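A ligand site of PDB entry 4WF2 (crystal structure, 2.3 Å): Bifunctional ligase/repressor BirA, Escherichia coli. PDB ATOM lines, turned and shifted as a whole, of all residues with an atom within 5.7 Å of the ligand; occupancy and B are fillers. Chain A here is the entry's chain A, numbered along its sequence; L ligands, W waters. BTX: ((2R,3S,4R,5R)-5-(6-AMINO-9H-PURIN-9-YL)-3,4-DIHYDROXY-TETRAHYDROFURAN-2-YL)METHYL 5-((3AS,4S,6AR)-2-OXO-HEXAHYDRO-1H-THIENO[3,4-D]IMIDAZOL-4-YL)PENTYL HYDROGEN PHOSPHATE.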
ATOM      1  N   ASP A  88     -27.774 -35.611 -27.142  1.00  0.00           N
ATOM      2  CA  ASP A  88     -27.528 -34.926 -25.871  1.00  0.00           C
ATOM      3  C   ASP A  88     -26.782 -33.617 -26.117  1.00  0.00           C
ATOM      4  O   ASP A  88     -27.136 -32.576 -25.559  1.00  0.00           O
ATOM      5  CB  ASP A  88     -26.752 -35.835 -24.899  1.00  0.00           C
ATOM      6  CG  ASP A  88     -25.394 -36.270 -25.449  1.00  0.00           C
ATOM      7  OD1 ASP A  88     -25.182 -36.210 -26.675  1.00  0.00           O
ATOM      8  OD2 ASP A  88     -24.544 -36.691 -24.630  1.00  0.00           O
ATOM      9  N   SER A  89     -25.767 -33.674 -26.977  1.00  0.00           N
ATOM     10  CA  SER A  89     -24.985 -32.490 -27.318  1.00  0.00           C
ATOM     11  C   SER A  89     -24.114 -32.817 -28.533  1.00  0.00           C
ATOM     12  O   SER A  89     -23.460 -33.861 -28.553  1.00  0.00           O
ATOM     13  CB  SER A  89     -24.116 -32.043 -26.132  1.00  0.00           C
ATOM     14  OG  SER A  89     -23.224 -31.014 -26.509  1.00  0.00           O
ATOM     15  N   THR A  90     -24.142 -31.947 -29.537  1.00  0.00           N
ATOM     16  CA  THR A  90     -23.347 -32.194 -30.740  1.00  0.00           C
ATOM     17  C   THR A  90     -21.863 -32.189 -30.404  1.00  0.00           C
ATOM     18  O   THR A  90     -21.073 -32.890 -31.025  1.00  0.00           O
ATOM     19  CB  THR A  90     -23.643 -31.160 -31.862  1.00  0.00           C
ATOM     20  OG1 THR A  90     -23.655 -29.835 -31.308  1.00  0.00           O
ATOM     21  CG2 THR A  90     -24.986 -31.453 -32.503  1.00  0.00           C
ATOM     22  N   ASN A  91     -21.482 -31.398 -29.403  1.00  0.00           N
ATOM     23  CA  ASN A  91     -20.105 -31.410 -28.932  1.00  0.00           C
ATOM     24  C   ASN A  91     -19.761 -32.753 -28.316  1.00  0.00           C
ATOM     25  O   ASN A  91     -18.691 -33.307 -28.566  1.00  0.00           O
ATOM     26  CB  ASN A  91     -19.874 -30.288 -27.912  1.00  0.00           C
ATOM     27  CG  ASN A  91     -19.283 -29.048 -28.546  1.00  0.00           C
ATOM     28  OD1 ASN A  91     -19.510 -28.761 -29.726  1.00  0.00           O
ATOM     29  ND2 ASN A  91     -18.508 -28.295 -27.769  1.00  0.00           N
ATOM     30  N   GLN A 112     -31.141 -30.699 -29.019  1.00  0.00           N
ATOM     31  CA  GLN A 112     -30.195 -31.128 -27.977  1.00  0.00           C
ATOM     32  C   GLN A 112     -30.902 -31.204 -26.621  1.00  0.00           C
ATOM     33  O   GLN A 112     -31.504 -30.229 -26.180  1.00  0.00           O
ATOM     34  CB  GLN A 112     -29.003 -30.162 -27.879  1.00  0.00           C
ATOM     35  CG  GLN A 112     -28.174 -30.080 -29.145  1.00  0.00           C
ATOM     36  CD  GLN A 112     -26.989 -29.145 -29.007  1.00  0.00           C
ATOM     37  OE1 GLN A 112     -25.859 -29.497 -29.353  1.00  0.00           O
ATOM     38  NE2 GLN A 112     -27.238 -27.947 -28.491  1.00  0.00           N
ATOM     39  N   ALA A 114     -29.264 -31.970 -23.811  1.00  0.00           N
ATOM     40  CA  ALA A 114     -28.288 -31.494 -22.826  1.00  0.00           C
ATOM     41  C   ALA A 114     -27.286 -30.545 -23.482  1.00  0.00           C
ATOM     42  O   ALA A 114     -26.068 -30.689 -23.293  1.00  0.00           O
ATOM     43  CB  ALA A 114     -27.572 -32.671 -22.175  1.00  0.00           C
ATOM     44  N   GLY A 115     -27.777 -29.596 -24.273  1.00  0.00           N
ATOM     45  CA  GLY A 115     -26.925 -28.600 -24.880  1.00  0.00           C
ATOM     46  C   GLY A 115     -26.358 -27.711 -23.803  1.00  0.00           C
ATOM     47  O   GLY A 115     -27.088 -27.298 -22.904  1.00  0.00           O
ATOM     48  N   ARG A 116     -25.062 -27.425 -23.885  1.00  0.00           N
ATOM     49  CA  ARG A 116     -24.408 -26.624 -22.860  1.00  0.00           C
ATOM     50  C   ARG A 116     -23.734 -25.381 -23.437  1.00  0.00           C
ATOM     51  O   ARG A 116     -23.321 -25.353 -24.603  1.00  0.00           O
ATOM     52  CB  ARG A 116     -23.397 -27.474 -22.098  1.00  0.00           C
ATOM     53  CG  ARG A 116     -22.222 -27.973 -22.924  1.00  0.00           C
ATOM     54  CD  ARG A 116     -21.473 -29.065 -22.167  1.00  0.00           C
ATOM     55  NE  ARG A 116     -20.382 -29.649 -22.945  1.00  0.00           N
ATOM     56  CZ  ARG A 116     -20.321 -30.918 -23.353  1.00  0.00           C
ATOM     57  NH1 ARG A 116     -21.284 -31.784 -23.079  1.00  0.00           N
ATOM     58  NH2 ARG A 116     -19.273 -31.327 -24.057  1.00  0.00           N
ATOM     59  N   GLY A 117     -23.663 -24.351 -22.604  1.00  0.00           N
ATOM     60  CA  GLY A 117     -22.882 -23.168 -22.901  1.00  0.00           C
ATOM     61  C   GLY A 117     -21.509 -23.315 -22.286  1.00  0.00           C
ATOM     62  O   GLY A 117     -20.994 -24.433 -22.137  1.00  0.00           O
ATOM     63  N   ARG A 118     -20.909 -22.189 -21.910  1.00  0.00           N
ATOM     64  CA  ARG A 118     -19.607 -22.195 -21.263  1.00  0.00           C
ATOM     65  C   ARG A 118     -19.758 -22.250 -19.752  1.00  0.00           C
ATOM     66  O   ARG A 118     -20.787 -21.866 -19.200  1.00  0.00           O
ATOM     67  CB  ARG A 118     -18.807 -20.956 -21.692  1.00  0.00           C
ATOM     68  CG  ARG A 118     -18.505 -20.919 -23.180  1.00  0.00           C
ATOM     69  CD  ARG A 118     -17.682 -19.698 -23.564  1.00  0.00           C
ATOM     70  NE  ARG A 118     -18.471 -18.473 -23.452  1.00  0.00           N
ATOM     71  CZ  ARG A 118     -19.175 -17.927 -24.442  1.00  0.00           C
ATOM     72  NH1 ARG A 118     -19.197 -18.458 -25.658  1.00  0.00           N
ATOM     73  NH2 ARG A 118     -19.849 -16.808 -24.198  1.00  0.00           N
ATOM     74  N   ARG A 119     -18.722 -22.761 -19.080  1.00  0.00           N
ATOM     75  CA  ARG A 119     -18.690 -22.839 -17.622  1.00  0.00           C
ATOM     76  C   ARG A 119     -19.883 -23.583 -17.026  1.00  0.00           C
ATOM     77  O   ARG A 119     -20.404 -23.191 -15.981  1.00  0.00           O
ATOM     78  CB  ARG A 119     -18.612 -21.430 -17.022  1.00  0.00           C
ATOM     79  CG  ARG A 119     -17.396 -20.644 -17.463  1.00  0.00           C
ATOM     80  CD  ARG A 119     -17.173 -19.431 -16.576  1.00  0.00           C
ATOM     81  NE  ARG A 119     -15.845 -19.422 -15.981  1.00  0.00           N
ATOM     82  CZ  ARG A 119     -15.536 -18.857 -14.813  1.00  0.00           C
ATOM     83  NH1 ARG A 119     -16.466 -18.249 -14.082  1.00  0.00           N
ATOM     84  NH2 ARG A 119     -14.289 -18.899 -14.370  1.00  0.00           N
ATOM     85  N   ARG A 121     -22.934 -23.875 -17.975  1.00  0.00           N
ATOM     86  CA  ARG A 121     -24.268 -23.353 -18.260  1.00  0.00           C
ATOM     87  C   ARG A 121     -24.942 -24.187 -19.344  1.00  0.00           C
ATOM     88  O   ARG A 121     -24.308 -25.023 -19.982  1.00  0.00           O
ATOM     89  CB  ARG A 121     -24.189 -21.889 -18.693  1.00  0.00           C
ATOM     90  CG  ARG A 121     -23.589 -20.975 -17.641  1.00  0.00           C
ATOM     91  CD  ARG A 121     -23.460 -19.552 -18.154  1.00  0.00           C
ATOM     92  NE  ARG A 121     -22.218 -18.927 -17.707  1.00  0.00           N
ATOM     93  CZ  ARG A 121     -21.233 -18.525 -18.504  1.00  0.00           C
ATOM     94  NH1 ARG A 121     -21.290 -18.646 -19.825  1.00  0.00           N
ATOM     95  NH2 ARG A 121     -20.146 -17.975 -17.966  1.00  0.00           N
ATOM     96  N   LYS A 122     -26.241 -23.954 -19.534  1.00  0.00           N
ATOM     97  CA  LYS A 122     -27.036 -24.706 -20.504  1.00  0.00           C
ATOM     98  C   LYS A 122     -27.361 -23.847 -21.716  1.00  0.00           C
ATOM     99  O   LYS A 122     -27.494 -22.625 -21.603  1.00  0.00           O
ATOM    100  CB  LYS A 122     -28.328 -25.223 -19.872  1.00  0.00           C
ATOM    101  CG  LYS A 122     -28.150 -25.672 -18.438  1.00  0.00           C
ATOM    102  CD  LYS A 122     -29.358 -26.468 -17.948  1.00  0.00           C
ATOM    103  CE  LYS A 122     -29.180 -26.887 -16.499  1.00  0.00           C
ATOM    104  NZ  LYS A 122     -27.848 -27.510 -16.249  1.00  0.00           N
ATOM    105  N   TRP A 123     -27.473 -24.494 -22.866  1.00  0.00           N
ATOM    106  CA  TRP A 123     -27.893 -23.842 -24.103  1.00  0.00           C
ATOM    107  C   TRP A 123     -29.254 -24.404 -24.518  1.00  0.00           C
ATOM    108  O   TRP A 123     -29.361 -25.546 -24.947  1.00  0.00           O
ATOM    109  CB  TRP A 123     -26.858 -24.054 -25.207  1.00  0.00           C
ATOM    110  CG  TRP A 123     -27.131 -23.238 -26.440  1.00  0.00           C
ATOM    111  CD1 TRP A 123     -27.690 -23.669 -27.606  1.00  0.00           C
ATOM    112  CD2 TRP A 123     -26.843 -21.847 -26.630  1.00  0.00           C
ATOM    113  NE1 TRP A 123     -27.773 -22.636 -28.511  1.00  0.00           N
ATOM    114  CE2 TRP A 123     -27.263 -21.506 -27.932  1.00  0.00           C
ATOM    115  CE3 TRP A 123     -26.281 -20.854 -25.820  1.00  0.00           C
ATOM    116  CZ2 TRP A 123     -27.129 -20.215 -28.443  1.00  0.00           C
ATOM    117  CZ3 TRP A 123     -26.158 -19.574 -26.327  1.00  0.00           C
ATOM    118  CH2 TRP A 123     -26.574 -19.264 -27.629  1.00  0.00           C
ATOM    119  N   PHE A 124     -30.300 -23.592 -24.356  1.00  0.00           N
ATOM    120  CA  PHE A 124     -31.646 -23.960 -24.766  1.00  0.00           C
ATOM    121  C   PHE A 124     -31.671 -24.276 -26.259  1.00  0.00           C
ATOM    122  O   PHE A 124     -31.372 -23.420 -27.099  1.00  0.00           O
ATOM    123  CB  PHE A 124     -32.640 -22.840 -24.444  1.00  0.00           C
ATOM    124  CG  PHE A 124     -34.077 -23.224 -24.665  1.00  0.00           C
ATOM    125  CD1 PHE A 124     -34.592 -24.371 -24.107  1.00  0.00           C
ATOM    126  CD2 PHE A 124     -34.905 -22.417 -25.435  1.00  0.00           C
ATOM    127  CE1 PHE A 124     -35.916 -24.729 -24.310  1.00  0.00           C
ATOM    128  CE2 PHE A 124     -36.228 -22.774 -25.638  1.00  0.00           C
ATOM    129  CZ  PHE A 124     -36.733 -23.930 -25.075  1.00  0.00           C
ATOM    130  N   SER A 125     -32.038 -25.519 -26.588  1.00  0.00           N
ATOM    131  CA  SER A 125     -31.904 -26.025 -27.945  1.00  0.00           C
ATOM    132  C   SER A 125     -33.166 -26.724 -28.422  1.00  0.00           C
ATOM    133  O   SER A 125     -33.140 -27.919 -28.682  1.00  0.00           O
ATOM    134  CB  SER A 125     -30.724 -27.000 -28.016  1.00  0.00           C
ATOM    135  OG  SER A 125     -29.547 -26.417 -27.483  1.00  0.00           O
ATOM    136  N   ASN A 130     -33.486 -23.782 -34.349  1.00  0.00           N
ATOM    137  CA  ASN A 130     -32.178 -23.169 -34.495  1.00  0.00           C
ATOM    138  C   ASN A 130     -31.158 -24.109 -35.117  1.00  0.00           C
ATOM    139  O   ASN A 130     -31.462 -25.273 -35.394  1.00  0.00           O
ATOM    140  CB  ASN A 130     -31.673 -22.699 -33.138  1.00  0.00           C
ATOM    141  CG  ASN A 130     -32.682 -21.860 -32.406  1.00  0.00           C
ATOM    142  OD1 ASN A 130     -33.006 -20.759 -32.830  1.00  0.00           O
ATOM    143  ND2 ASN A 130     -33.181 -22.386 -31.289  1.00  0.00           N
ATOM    144  N   LEU A 131     -29.935 -23.609 -35.309  1.00  0.00           N
ATOM    145  CA  LEU A 131     -28.846 -24.440 -35.792  1.00  0.00           C
ATOM    146  C   LEU A 131     -27.914 -24.833 -34.652  1.00  0.00           C
ATOM    147  O   LEU A 131     -27.365 -23.961 -33.974  1.00  0.00           O
ATOM    148  CB  LEU A 131     -28.060 -23.719 -36.895  1.00  0.00           C
ATOM    149  CG  LEU A 131     -27.048 -24.609 -37.619  1.00  0.00           C
ATOM    150  CD1 LEU A 131     -27.733 -25.763 -38.352  1.00  0.00           C
ATOM    151  CD2 LEU A 131     -26.215 -23.782 -38.584  1.00  0.00           C
ATOM    152  N   TYR A 132     -27.759 -26.138 -34.431  1.00  0.00           N
ATOM    153  CA  TYR A 132     -26.798 -26.675 -33.471  1.00  0.00           C
ATOM    154  C   TYR A 132     -25.773 -27.521 -34.230  1.00  0.00           C
ATOM    155  O   TYR A 132     -26.056 -28.629 -34.661  1.00  0.00           O
ATOM    156  CB  TYR A 132     -27.506 -27.515 -32.395  1.00  0.00           C
ATOM    157  CG  TYR A 132     -28.840 -26.932 -31.988  1.00  0.00           C
ATOM    158  CD1 TYR A 132     -28.914 -25.698 -31.362  1.00  0.00           C
ATOM    159  CD2 TYR A 132     -30.033 -27.603 -32.242  1.00  0.00           C
ATOM    160  CE1 TYR A 132     -30.128 -25.148 -30.996  1.00  0.00           C
ATOM    161  CE2 TYR A 132     -31.255 -27.064 -31.882  1.00  0.00           C
ATOM    162  CZ  TYR A 132     -31.300 -25.836 -31.263  1.00  0.00           C
ATOM    163  OH  TYR A 132     -32.506 -25.284 -30.893  1.00  0.00           O
ATOM    164  N   LEU A 133     -24.576 -26.945 -34.394  1.00  0.00           N
ATOM    165  CA  LEU A 133     -23.535 -27.545 -35.223  1.00  0.00           C
ATOM    166  C   LEU A 133     -22.249 -27.728 -34.442  1.00  0.00           C
ATOM    167  O   LEU A 133     -21.882 -26.886 -33.615  1.00  0.00           O
ATOM    168  CB  LEU A 133     -23.283 -26.670 -36.463  1.00  0.00           C
ATOM    169  CG  LEU A 133     -21.953 -26.803 -37.205  1.00  0.00           C
ATOM    170  CD1 LEU A 133     -21.856 -28.133 -37.954  1.00  0.00           C
ATOM    171  CD2 LEU A 133     -21.772 -25.640 -38.160  1.00  0.00           C
ATOM    172  N   SER A 134     -21.554 -28.822 -34.729  1.00  0.00           N
ATOM    173  CA  SER A 134     -20.241 -29.069 -34.145  1.00  0.00           C
ATOM    174  C   SER A 134     -19.275 -29.627 -35.182  1.00  0.00           C
ATOM    175  O   SER A 134     -19.704 -30.294 -36.129  1.00  0.00           O
ATOM    176  CB  SER A 134     -20.353 -30.024 -32.951  1.00  0.00           C
ATOM    177  OG  SER A 134     -21.079 -29.440 -31.896  1.00  0.00           O
ATOM    178  N   ASN A 175     -15.815 -15.056 -28.613  1.00  0.00           N
ATOM    179  CA  ASN A 175     -16.579 -16.217 -28.933  1.00  0.00           C
ATOM    180  C   ASN A 175     -18.105 -16.183 -28.934  1.00  0.00           C
ATOM    181  O   ASN A 175     -18.748 -17.203 -28.718  1.00  0.00           O
ATOM    182  CB  ASN A 175     -16.187 -17.236 -27.905  1.00  0.00           C
ATOM    183  CG  ASN A 175     -16.578 -16.829 -26.537  1.00  0.00           C
ATOM    184  OD1 ASN A 175     -17.259 -15.862 -26.345  1.00  0.00           O
ATOM    185  ND2 ASN A 175     -16.118 -17.542 -25.604  1.00  0.00           N
ATOM    186  N   ASP A 176     -18.715 -15.058 -29.202  1.00  0.00           N
ATOM    187  CA  ASP A 176     -20.134 -14.975 -29.323  1.00  0.00           C
ATOM    188  C   ASP A 176     -20.412 -14.130 -30.534  1.00  0.00           C
ATOM    189  O   ASP A 176     -19.646 -13.272 -30.847  1.00  0.00           O
ATOM    190  CB  ASP A 176     -20.780 -14.444 -28.047  1.00  0.00           C
ATOM    191  CG  ASP A 176     -20.938 -15.515 -26.969  1.00  0.00           C
ATOM    192  OD1 ASP A 176     -20.947 -16.675 -27.279  1.00  0.00           O
ATOM    193  OD2 ASP A 176     -21.043 -15.184 -25.807  1.00  0.00           O
ATOM    194  N   LYS A 183     -27.158 -11.340 -27.710  1.00  0.00           N
ATOM    195  CA  LYS A 183     -26.523 -12.615 -28.071  1.00  0.00           C
ATOM    196  C   LYS A 183     -27.325 -13.357 -29.136  1.00  0.00           C
ATOM    197  O   LYS A 183     -28.424 -13.859 -28.877  1.00  0.00           O
ATOM    198  CB  LYS A 183     -26.358 -13.499 -26.834  1.00  0.00           C
ATOM    199  CG  LYS A 183     -25.466 -14.716 -27.072  1.00  0.00           C
ATOM    200  CD  LYS A 183     -25.650 -15.791 -26.009  1.00  0.00           C
ATOM    201  CE  LYS A 183     -24.888 -15.473 -24.744  1.00  0.00           C
ATOM    202  NZ  LYS A 183     -23.415 -15.613 -24.952  1.00  0.00           N
ATOM    203  N   LEU A 184     -26.742 -13.434 -30.333  1.00  0.00           N
ATOM    204  CA  LEU A 184     -27.359 -14.127 -31.453  1.00  0.00           C
ATOM    205  C   LEU A 184     -26.921 -15.588 -31.516  1.00  0.00           C
ATOM    206  O   LEU A 184     -27.719 -16.472 -31.804  1.00  0.00           O
ATOM    207  CB  LEU A 184     -27.020 -13.420 -32.765  1.00  0.00           C
ATOM    208  CG  LEU A 184     -27.385 -14.143 -34.059  1.00  0.00           C
ATOM    209  CD1 LEU A 184     -28.893 -14.317 -34.185  1.00  0.00           C
ATOM    210  CD2 LEU A 184     -26.832 -13.386 -35.250  1.00  0.00           C
ATOM    211  N   GLY A 186     -23.801 -18.582 -29.851  1.00  0.00           N
ATOM    212  CA  GLY A 186     -22.785 -18.939 -28.891  1.00  0.00           C
ATOM    213  C   GLY A 186     -21.802 -19.957 -29.426  1.00  0.00           C
ATOM    214  O   GLY A 186     -22.187 -20.936 -30.082  1.00  0.00           O
ATOM    215  N   ILE A 187     -20.520 -19.738 -29.156  1.00  0.00           N
ATOM    216  CA  ILE A 187     -19.455 -20.634 -29.578  1.00  0.00           C
ATOM    217  C   ILE A 187     -18.783 -21.269 -28.363  1.00  0.00           C
ATOM    218  O   ILE A 187     -18.367 -20.573 -27.443  1.00  0.00           O
ATOM    219  CB  ILE A 187     -18.368 -19.903 -30.415  1.00  0.00           C
ATOM    220  CG1 ILE A 187     -18.982 -19.309 -31.683  1.00  0.00           C
ATOM    221  CG2 ILE A 187     -17.218 -20.847 -30.772  1.00  0.00           C
ATOM    222  CD1 ILE A 187     -18.038 -18.378 -32.418  1.00  0.00           C
ATOM    223  N   LEU A 188     -18.688 -22.600 -28.381  1.00  0.00           N
ATOM    224  CA  LEU A 188     -18.001 -23.351 -27.351  1.00  0.00           C
ATOM    225  C   LEU A 188     -16.894 -24.207 -27.964  1.00  0.00           C
ATOM    226  O   LEU A 188     -17.168 -25.138 -28.726  1.00  0.00           O
ATOM    227  CB  LEU A 188     -18.984 -24.238 -26.577  1.00  0.00           C
ATOM    228  CG  LEU A 188     -18.412 -25.219 -25.550  1.00  0.00           C
ATOM    229  CD1 LEU A 188     -17.735 -24.477 -24.405  1.00  0.00           C
ATOM    230  CD2 LEU A 188     -19.504 -26.139 -25.009  1.00  0.00           C
ATOM    231  N   GLY A 204     -18.129 -26.024 -31.192  1.00  0.00           N
ATOM    232  CA  GLY A 204     -19.573 -26.020 -31.083  1.00  0.00           C
ATOM    233  C   GLY A 204     -20.163 -24.649 -31.305  1.00  0.00           C
ATOM    234  O   GLY A 204     -19.732 -23.663 -30.692  1.00  0.00           O
ATOM    235  N   ALA A 205     -21.139 -24.570 -32.203  1.00  0.00           N
ATOM    236  CA  ALA A 205     -21.815 -23.322 -32.529  1.00  0.00           C
ATOM    237  C   ALA A 205     -23.342 -23.481 -32.458  1.00  0.00           C
ATOM    238  O   ALA A 205     -23.913 -24.366 -33.092  1.00  0.00           O
ATOM    239  CB  ALA A 205     -21.402 -22.845 -33.914  1.00  0.00           C
ATOM    240  N   GLY A 206     -23.970 -22.606 -31.675  1.00  0.00           N
ATOM    241  CA  GLY A 206     -25.410 -22.530 -31.592  1.00  0.00           C
ATOM    242  C   GLY A 206     -25.864 -21.175 -32.096  1.00  0.00           C
ATOM    243  O   GLY A 206     -25.510 -20.149 -31.520  1.00  0.00           O
ATOM    244  N   ASN A 208     -29.130 -18.779 -33.052  1.00  0.00           N
ATOM    245  CA  ASN A 208     -30.567 -18.562 -32.907  1.00  0.00           C
ATOM    246  C   ASN A 208     -31.204 -18.072 -34.210  1.00  0.00           C
ATOM    247  O   ASN A 208     -30.820 -17.025 -34.734  1.00  0.00           O
ATOM    248  CB  ASN A 208     -30.845 -17.568 -31.788  1.00  0.00           C
ATOM    249  CG  ASN A 208     -30.313 -18.034 -30.448  1.00  0.00           C
ATOM    250  OD1 ASN A 208     -30.295 -19.229 -30.154  1.00  0.00           O
ATOM    251  ND2 ASN A 208     -29.848 -17.086 -29.638  1.00  0.00           N
ATOM    252  N   MET A 211     -36.674 -19.437 -32.977  1.00  0.00           N
ATOM    253  CA  MET A 211     -36.958 -19.490 -31.538  1.00  0.00           C
ATOM    254  C   MET A 211     -38.014 -18.472 -31.099  1.00  0.00           C
ATOM    255  O   MET A 211     -39.020 -18.823 -30.525  1.00  0.00           O
ATOM    256  CB  MET A 211     -35.665 -19.369 -30.701  1.00  0.00           C
ATOM    257  CG  MET A 211     -35.873 -19.493 -29.193  1.00  0.00           C
ATOM    258  SD  MET A 211     -34.432 -19.485 -28.116  1.00  0.00           S
ATOM    259  CE  MET A 211     -33.886 -21.139 -28.344  1.00  0.00           C
ATOM    260  N   TRP A 223     -31.255 -12.212 -25.401  1.00  0.00           N
ATOM    261  CA  TRP A 223     -30.909 -12.900 -26.638  1.00  0.00           C
ATOM    262  C   TRP A 223     -31.602 -12.248 -27.818  1.00  0.00           C
ATOM    263  O   TRP A 223     -32.404 -11.319 -27.650  1.00  0.00           O
ATOM    264  CB  TRP A 223     -31.262 -14.400 -26.574  1.00  0.00           C
ATOM    265  CG  TRP A 223     -32.517 -14.761 -25.839  1.00  0.00           C
ATOM    266  CD1 TRP A 223     -32.662 -14.873 -24.490  1.00  0.00           C
ATOM    267  CD2 TRP A 223     -33.790 -15.085 -26.411  1.00  0.00           C
ATOM    268  NE1 TRP A 223     -33.953 -15.244 -24.186  1.00  0.00           N
ATOM    269  CE2 TRP A 223     -34.662 -15.373 -25.347  1.00  0.00           C
ATOM    270  CE3 TRP A 223     -34.275 -15.159 -27.719  1.00  0.00           C
ATOM    271  CZ2 TRP A 223     -35.999 -15.733 -25.546  1.00  0.00           C
ATOM    272  CZ3 TRP A 223     -35.600 -15.507 -27.922  1.00  0.00           C
ATOM    273  CH2 TRP A 223     -36.446 -15.791 -26.844  1.00  0.00           C
HETATM  274  P   BTX L   1     -23.232 -19.388 -22.842  1.00  0.00           P
HETATM  275  O1P BTX L   1     -22.584 -19.937 -21.585  1.00  0.00           O
HETATM  276  O2P BTX L   1     -22.893 -17.976 -23.253  1.00  0.00           O
HETATM  277  O5' BTX L   1     -24.812 -19.456 -22.677  1.00  0.00           O
HETATM  278  C5' BTX L   1     -25.422 -19.959 -21.492  1.00  0.00           C
HETATM  279  C4' BTX L   1     -26.265 -18.913 -20.821  1.00  0.00           C
HETATM  280  O4' BTX L   1     -26.931 -18.128 -21.836  1.00  0.00           O
HETATM  281  C3' BTX L   1     -27.342 -19.462 -19.882  1.00  0.00           C
HETATM  282  O3' BTX L   1     -27.056 -19.034 -18.556  1.00  0.00           O
HETATM  283  C2' BTX L   1     -28.658 -18.803 -20.337  1.00  0.00           C
HETATM  284  O2' BTX L   1     -29.131 -17.805 -19.470  1.00  0.00           O
HETATM  285  C1' BTX L   1     -28.335 -18.239 -21.728  1.00  0.00           C
HETATM  286  N9  BTX L   1     -28.841 -19.037 -22.855  1.00  0.00           N
HETATM  287  C8  BTX L   1     -29.262 -20.325 -22.784  1.00  0.00           C
HETATM  288  N7  BTX L   1     -29.661 -20.690 -24.028  1.00  0.00           N
HETATM  289  C5  BTX L   1     -29.495 -19.641 -24.865  1.00  0.00           C
HETATM  290  C6  BTX L   1     -29.747 -19.477 -26.218  1.00  0.00           C
HETATM  291  N6  BTX L   1     -30.259 -20.328 -27.238  1.00  0.00           N
HETATM  292  N1  BTX L   1     -29.493 -18.298 -26.812  1.00  0.00           N
HETATM  293  C2  BTX L   1     -28.977 -17.250 -26.078  1.00  0.00           C
HETATM  294  N3  BTX L   1     -28.726 -17.404 -24.747  1.00  0.00           N
HETATM  295  C4  BTX L   1     -28.995 -18.606 -24.141  1.00  0.00           C
HETATM  296  CBB BTX L   1     -22.256 -19.925 -25.252  1.00  0.00           C
HETATM  297  OBB BTX L   1     -22.868 -20.388 -24.031  1.00  0.00           O
HETATM  298  CAB BTX L   1     -21.829 -21.132 -26.107  1.00  0.00           C
HETATM  299  C9B BTX L   1     -23.070 -21.908 -26.602  1.00  0.00           C
HETATM  300  C8B BTX L   1     -22.640 -23.188 -27.360  1.00  0.00           C
HETATM  301  C7B BTX L   1     -23.898 -23.905 -27.858  1.00  0.00           C
HETATM  302  C2B BTX L   1     -23.527 -24.883 -29.086  1.00  0.00           C
HETATM  303  S1B BTX L   1     -24.899 -25.555 -29.745  1.00  0.00           S
HETATM  304  C6B BTX L   1     -24.236 -26.869 -30.562  1.00  0.00           C
HETATM  305  C5B BTX L   1     -23.098 -27.287 -29.701  1.00  0.00           C
HETATM  306  N1B BTX L   1     -23.530 -28.314 -28.972  1.00  0.00           N
HETATM  307  C3B BTX L   1     -23.497 -27.876 -27.463  1.00  0.00           C
HETATM  308  O3B BTX L   1     -23.821 -28.565 -26.495  1.00  0.00           O
HETATM  309  N2B BTX L   1     -22.965 -26.421 -27.423  1.00  0.00           N
HETATM  310  C4B BTX L   1     -22.728 -26.043 -28.673  1.00  0.00           C
HETATM  311  O   HOH W   1     -27.690 -16.599 -16.623  1.00  0.00           O
HETATM  312  O   HOH W   2     -31.096 -15.355 -19.774  1.00  0.00           O
HETATM  313  O   HOH W   3     -27.570 -21.914 -17.764  1.00  0.00           O
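The guanidinium group of Arg 118 lies within salt-bridge range of an oxygen (O2P) of the ligand, at 3.4 Å. The backbone carbonyl oxygen (O) of Arg 116 is in hydrogen-bond range of a nitrogen (N2B) of the ligand, at 3.0 Å. The side-chain hydroxyl (OG) of Ser 89 sits at hydrogen-bond distance from an oxygen (O3B) of the ligand (2.5 Å). NZ of Lys 183 is in salt-bridge range of O2P of the ligand. N1B of the ligand is in hydrogen-bond range of OE1 of Gln 112 (2.6 Å). The backbone carbonyl oxygen (O) of Phe 124 is in hydrogen-bond range of a nitrogen (N6) of the ligand (3.3 Å). S1B of the ligand lies close to N of Gly 206 (3.6 Å). An oxygen (O1P) of the ligand lies within salt-bridge range of the guanidinium group (NH1) of Arg 121 (2.5 Å). N1B of the ligand is in hydrogen-bond range of OG1 of Thr 90, at 2.8 Å. N1 of the ligand lies within hydrogen-bond range of ND2 of Asn 208, 3.1 Å away. N7 of the ligand lies within hydrogen-bond range of N of Phe 124, at 3.0 Å. An oxygen (O3B) of the ligand sits at hydrogen-bond distance from the backbone NH (N) of Arg 116 (3.1 Å). An oxygen (O1P) of the ligand sits at hydrogen-bond distance from the backbone NH (N) of Arg 118, 2.8 Å away.
Water W3 lies within hydrogen-bond range of N of Lys 122 and O3' of the ligand.
The backbone carbonyl oxygen (O) of Ala 205 lies close to a sulfur (S1B) of the ligand, at 3.7 Å. Merely in contact with the ligand: Asn 91, Gly 115, Gly 117, Lys 122, Trp 123, Tyr 132, Leu 133, Ser 134, Gly 186, Ile 187, Leu 188, Gly 204, Met 211 and Trp 223. 25 residues have an atom within 4 Å of the ligand: Ser 89, Thr 90, Asn 91, Gln 112, Gly 115, Arg 116, Gly 117, Arg 118, Arg 121, Lys 122, Trp 123, Phe 124, Tyr 132, Leu 133, Ser 134, Lys 183, Gly 186, Ile 187, Leu 188, Gly 204, Ala 205, Gly 206, Asn 208, Met 211 and Trp 223. The nearest printed residue that does not touch the ligand is Asp 176 (4.05 Å).
NH1 of Arg 118 sits at hydrogen-bond distance from O of Ile 187 (2.9 Å). The side-chain carboxylate (OD2) of Asp 176 is in salt-bridge range of the side-chain amino group (NZ) of Lys 183, at 2.6 Å. The backbone NH (N) of Leu 188 sits at hydrogen-bond distance from the backbone carbonyl oxygen (O) of Gly 204 (2.7 Å). N of Gly 115 sits at hydrogen-bond distance from O of Asp 88. The backbone NH (N) of Asn 208 is in hydrogen-bond range of the backbone carbonyl oxygen (O) of Leu 184, at 3.0 Å. The side-chain hydroxyl (OG) of Ser 125 is in hydrogen-bond range of the backbone carbonyl oxygen (O) of Trp 123 (2.7 Å). The backbone NH (N) of Ile 187 sits at hydrogen-bond distance from the backbone carbonyl oxygen (O) of Asn 175 (3.1 Å). ND2 of Asn 130 lies within hydrogen-bond range of OH of Tyr 132 (3.0 Å).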
